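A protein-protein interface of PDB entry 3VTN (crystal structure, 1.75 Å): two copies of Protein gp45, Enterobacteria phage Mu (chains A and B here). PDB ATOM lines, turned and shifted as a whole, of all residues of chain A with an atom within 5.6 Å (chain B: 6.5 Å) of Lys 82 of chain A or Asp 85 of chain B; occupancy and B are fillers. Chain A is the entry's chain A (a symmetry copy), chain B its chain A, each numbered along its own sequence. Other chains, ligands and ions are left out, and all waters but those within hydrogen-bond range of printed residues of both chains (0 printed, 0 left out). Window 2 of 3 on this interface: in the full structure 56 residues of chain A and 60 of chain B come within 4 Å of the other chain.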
ATOM      1  N   ALA A  77      24.066  33.745  -0.687  1.00  0.00           N
ATOM      2  CA  ALA A  77      24.366  33.155   0.611  1.00  0.00           C
ATOM      3  C   ALA A  77      25.874  33.187   0.852  1.00  0.00           C
ATOM      4  O   ALA A  77      26.624  32.527   0.153  1.00  0.00           O
ATOM      5  CB  ALA A  77      23.823  31.732   0.685  1.00  0.00           C
ATOM      6  N   ILE A  78      26.316  33.965   1.835  1.00  0.00           N
ATOM      7  CA  ILE A  78      27.752  34.109   2.110  1.00  0.00           C
ATOM      8  C   ILE A  78      28.239  33.029   3.087  1.00  0.00           C
ATOM      9  O   ILE A  78      28.154  33.196   4.312  1.00  0.00           O
ATOM     10  CB  ILE A  78      28.113  35.536   2.600  1.00  0.00           C
ATOM     11  CG1 ILE A  78      27.426  36.617   1.749  1.00  0.00           C
ATOM     12  CG2 ILE A  78      29.613  35.733   2.643  1.00  0.00           C
ATOM     13  CD1 ILE A  78      27.659  36.534   0.241  1.00  0.00           C
ATOM     14  N   ILE A  79      28.751  31.928   2.524  1.00  0.00           N
ATOM     15  CA  ILE A  79      29.106  30.712   3.268  1.00  0.00           C
ATOM     16  C   ILE A  79      30.586  30.672   3.659  1.00  0.00           C
ATOM     17  O   ILE A  79      31.456  30.745   2.796  1.00  0.00           O
ATOM     18  CB  ILE A  79      28.743  29.418   2.467  1.00  0.00           C
ATOM     19  CG1 ILE A  79      27.263  29.408   2.037  1.00  0.00           C
ATOM     20  CG2 ILE A  79      29.110  28.157   3.249  1.00  0.00           C
ATOM     21  CD1 ILE A  79      26.250  29.562   3.173  1.00  0.00           C
ATOM     22  N   ASN A  80      30.852  30.546   4.960  1.00  0.00           N
ATOM     23  CA  ASN A  80      32.202  30.666   5.516  1.00  0.00           C
ATOM     24  C   ASN A  80      32.990  31.824   4.897  1.00  0.00           C
ATOM     25  O   ASN A  80      34.185  31.704   4.636  1.00  0.00           O
ATOM     26  CB  ASN A  80      32.972  29.341   5.382  1.00  0.00           C
ATOM     27  CG  ASN A  80      34.306  29.341   6.140  1.00  0.00           C
ATOM     28  OD1 ASN A  80      34.608  30.260   6.912  1.00  0.00           O
ATOM     29  ND2 ASN A  80      35.110  28.295   5.920  1.00  0.00           N
ATOM     30  N   GLY A  81      32.309  32.938   4.646  1.00  0.00           N
ATOM     31  CA  GLY A  81      32.955  34.124   4.092  1.00  0.00           C
ATOM     32  C   GLY A  81      33.021  34.181   2.577  1.00  0.00           C
ATOM     33  O   GLY A  81      33.557  35.147   2.010  1.00  0.00           O
ATOM     34  N   LYS A  82      32.457  33.169   1.924  1.00  0.00           N
ATOM     35  CA  LYS A  82      32.495  33.048   0.473  1.00  0.00           C
ATOM     36  C   LYS A  82      31.125  33.202  -0.178  1.00  0.00           C
ATOM     37  O   LYS A  82      30.150  32.634   0.296  1.00  0.00           O
ATOM     38  CB  LYS A  82      33.064  31.681   0.095  1.00  0.00           C
ATOM     39  CG  LYS A  82      34.533  31.471   0.443  1.00  0.00           C
ATOM     40  CD  LYS A  82      34.893  30.010   0.312  1.00  0.00           C
ATOM     41  CE  LYS A  82      34.506  29.238   1.548  1.00  0.00           C
ATOM     42  NZ  LYS A  82      33.879  27.937   1.203  1.00  0.00           N
ATOM     43  N   SER A  83      31.061  33.943  -1.283  1.00  0.00           N
ATOM     44  CA  SER A  83      29.833  34.087  -2.084  1.00  0.00           C
ATOM     45  C   SER A  83      29.399  32.767  -2.718  1.00  0.00           C
ATOM     46  O   SER A  83      30.238  31.974  -3.122  1.00  0.00           O
ATOM     47  CB  SER A  83      30.037  35.143  -3.169  1.00  0.00           C
ATOM     48  OG  SER A  83      28.912  35.231  -4.027  1.00  0.00           O
ATOM     49  N   THR A  84      28.091  32.534  -2.797  1.00  0.00           N
ATOM     50  CA  THR A  84      27.543  31.304  -3.388  1.00  0.00           C
ATOM     51  C   THR A  84      27.066  31.558  -4.819  1.00  0.00           C
ATOM     52  O   THR A  84      27.153  30.680  -5.679  1.00  0.00           O
ATOM     53  CB  THR A  84      26.381  30.701  -2.523  1.00  0.00           C
ATOM     54  OG1 THR A  84      26.890  30.257  -1.256  1.00  0.00           O
ATOM     55  CG2 THR A  84      25.710  29.515  -3.222  1.00  0.00           C
ATOM     56  N   PRO B  75      27.995  30.124   8.553  1.00  0.00           N
ATOM     57  CA  PRO B  75      29.277  29.400   8.538  1.00  0.00           C
ATOM     58  C   PRO B  75      29.261  28.254   7.525  1.00  0.00           C
ATOM     59  O   PRO B  75      30.273  28.001   6.854  1.00  0.00           O
ATOM     60  CB  PRO B  75      29.403  28.853   9.959  1.00  0.00           C
ATOM     61  CG  PRO B  75      28.034  28.971  10.556  1.00  0.00           C
ATOM     62  CD  PRO B  75      27.391  30.120   9.895  1.00  0.00           C
ATOM     63  N   ASP B  76      28.123  27.575   7.421  1.00  0.00           N
ATOM     64  CA  ASP B  76      27.913  26.541   6.419  1.00  0.00           C
ATOM     65  C   ASP B  76      26.419  26.363   6.168  1.00  0.00           C
ATOM     66  O   ASP B  76      25.593  26.702   7.022  1.00  0.00           O
ATOM     67  CB  ASP B  76      28.529  25.202   6.858  1.00  0.00           C
ATOM     68  CG  ASP B  76      28.801  24.254   5.680  1.00  0.00           C
ATOM     69  OD1 ASP B  76      28.462  24.590   4.527  1.00  0.00           O
ATOM     70  OD2 ASP B  76      29.354  23.162   5.903  1.00  0.00           O
ATOM     71  N   ALA B  77      26.080  25.833   4.997  1.00  0.00           N
ATOM     72  CA  ALA B  77      24.700  25.510   4.661  1.00  0.00           C
ATOM     73  C   ALA B  77      24.613  24.054   4.204  1.00  0.00           C
ATOM     74  O   ALA B  77      25.160  23.699   3.174  1.00  0.00           O
ATOM     75  CB  ALA B  77      24.177  26.460   3.590  1.00  0.00           C
ATOM     76  N   LYS B  82      24.167  17.751   2.067  1.00  0.00           N
ATOM     77  CA  LYS B  82      25.523  18.020   1.604  1.00  0.00           C
ATOM     78  C   LYS B  82      26.067  19.362   2.084  1.00  0.00           C
ATOM     79  O   LYS B  82      25.367  20.363   2.034  1.00  0.00           O
ATOM     80  CB  LYS B  82      25.546  18.002   0.076  1.00  0.00           C
ATOM     81  CG  LYS B  82      25.286  16.642  -0.561  1.00  0.00           C
ATOM     82  CD  LYS B  82      25.029  16.804  -2.040  1.00  0.00           C
ATOM     83  CE  LYS B  82      23.594  17.187  -2.308  1.00  0.00           C
ATOM     84  NZ  LYS B  82      23.500  18.253  -3.338  1.00  0.00           N
ATOM     85  N   SER B  83      27.326  19.383   2.517  1.00  0.00           N
ATOM     86  CA  SER B  83      28.023  20.621   2.902  1.00  0.00           C
ATOM     87  C   SER B  83      28.216  21.567   1.718  1.00  0.00           C
ATOM     88  O   SER B  83      28.451  21.118   0.605  1.00  0.00           O
ATOM     89  CB  SER B  83      29.376  20.289   3.527  1.00  0.00           C
ATOM     90  OG  SER B  83      30.120  21.461   3.811  1.00  0.00           O
ATOM     91  N   THR B  84      28.110  22.871   1.960  1.00  0.00           N
ATOM     92  CA  THR B  84      28.276  23.885   0.908  1.00  0.00           C
ATOM     93  C   THR B  84      29.672  24.507   0.974  1.00  0.00           C
ATOM     94  O   THR B  84      30.252  24.867  -0.052  1.00  0.00           O
ATOM     95  CB  THR B  84      27.177  25.002   0.985  1.00  0.00           C
ATOM     96  OG1 THR B  84      25.886  24.442   0.698  1.00  0.00           O
ATOM     97  CG2 THR B  84      27.447  26.135  -0.008  1.00  0.00           C
ATOM     98  N   ASP B  85      30.187  24.641   2.193  1.00  0.00           N
ATOM     99  CA  ASP B  85      31.550  25.103   2.458  1.00  0.00           C
ATOM    100  C   ASP B  85      32.605  24.135   1.873  1.00  0.00           C
ATOM    101  O   ASP B  85      33.705  24.550   1.496  1.00  0.00           O
ATOM    102  CB  ASP B  85      31.739  25.243   3.980  1.00  0.00           C
ATOM    103  CG  ASP B  85      33.110  25.772   4.373  1.00  0.00           C
ATOM    104  OD1 ASP B  85      33.645  26.661   3.677  1.00  0.00           O
ATOM    105  OD2 ASP B  85      33.640  25.307   5.407  1.00  0.00           O
ATOM    106  N   LYS B  86      32.245  22.855   1.792  1.00  0.00           N
ATOM    107  CA  LYS B  86      33.200  21.784   1.511  1.00  0.00           C
ATOM    108  C   LYS B  86      32.822  20.877   0.330  1.00  0.00           C
ATOM    109  O   LYS B  86      33.408  19.803   0.168  1.00  0.00           O
ATOM    110  CB  LYS B  86      33.399  20.927   2.773  1.00  0.00           C
ATOM    111  CG  LYS B  86      34.188  21.601   3.895  1.00  0.00           C
ATOM    112  CD  LYS B  86      34.301  20.704   5.116  1.00  0.00           C
ATOM    113  CE  LYS B  86      32.994  20.655   5.910  1.00  0.00           C
ATOM    114  NZ  LYS B  86      32.966  19.545   6.909  1.00  0.00           N
ATOM    115  N   HIS B  87      31.864  21.297  -0.493  1.00  0.00           N
ATOM    116  CA  HIS B  87      31.403  20.467  -1.609  1.00  0.00           C
ATOM    117  C   HIS B  87      32.377  20.437  -2.797  1.00  0.00           C
ATOM    118  O   HIS B  87      32.868  21.474  -3.256  1.00  0.00           O
ATOM    119  CB  HIS B  87      29.997  20.877  -2.056  1.00  0.00           C
ATOM    120  CG  HIS B  87      29.944  22.157  -2.830  1.00  0.00           C
ATOM    121  ND1 HIS B  87      30.485  23.337  -2.367  1.00  0.00           N
ATOM    122  CD2 HIS B  87      29.385  22.447  -4.028  1.00  0.00           C
ATOM    123  CE1 HIS B  87      30.276  24.294  -3.252  1.00  0.00           C
ATOM    124  NE2 HIS B  87      29.615  23.780  -4.273  1.00  0.00           N
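The backbone carbonyl oxygen of Pro 75 of chain B sits at hydrogen-bond distance from the backbone NH of Asn 80 of chain A (3.2 Å). The side-chain amide nitrogen (ND2) of Asn 80 of chain A sits at hydrogen-bond distance from the side-chain carboxylate (OD1) of Asp 85 of chain B (3.1 Å). NZ of Lys 82 of chain A lies within salt-bridge range of OD1 of Asp 85 of chain B (2.8 Å).
OG of Ser 83 of chain B sits at hydrogen-bond distance from OD2 of Asp 76 of chain B, at 2.8 Å. The side-chain carboxylate of Asp 76 of chain B sits at hydrogen-bond distance from the backbone NH of Thr 84 of chain B. The side-chain carboxylate (OD1) of Asp 76 of chain B lies within hydrogen-bond range of the backbone NH (N) of Asp 85 of chain B, 2.9 Å away. The backbone carbonyl oxygen of Ala 77 of chain B lies within hydrogen-bond range of the side-chain hydroxyl of Thr 84 of chain B (2.7 Å). The backbone carbonyl oxygen (O) of Thr 84 of chain B lies within hydrogen-bond range of a ring nitrogen (ND1) of His 87 of chain B.
Pro 75 of chain B touches Ile 79 of chain A (O to CG2, 3.8 Å). Asp 76 of chain B touches Ile 79 of chain A (CA to CG2, 3.8 Å). Ala 77 of chain B touches Ile 79 of chain A. Ile 79 of chain A touches Thr 84 of chain B (CG1 to CG2, 3.9 Å). Ile 79 of chain A touches Asp 85 of chain B.
Ile 78 of chain A touches none of the printed residues of chain B. Lys 82 of chain A touches one residue of chain B. Of the printed residues of chain A, Asp 76 of chain B touches Ile 79. Ser 83 of chain B touches none of the printed residues of chain A. Of the printed residues of chain A, Thr 84 of chain B touches Ile 79 (3.9 Å). Of chain A, only Ile 79 (3.8 Å), Asn 80 (3.1 Å) and Lys 82 (2.8 Å) come within 4 Å of Asp 85 of chain B. The nearest printed residue of chain A that does not touch Asp 85 of chain B is Gly 81 of chain A (6.5 Å). The nearest printed residue of chain A that does not touch Ala 77 of chain B is Ala 77 of chain A (6.0 Å).
Of the 9 printed residues of chain B, 5 touch a printed residue of chain A. Hydrophobic or aromatic side chains of chain B within 4 Å of the printed part of chain A: Ala 77. Of the 8 printed residues of chain A, 3 touch a printed residue of chain B.
Positions printed for both chains: 77, 82, 83 and 84. Of the 8 pairs that touch across the chains among the printed residues, none has its exchanged pair printed and touching as well.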
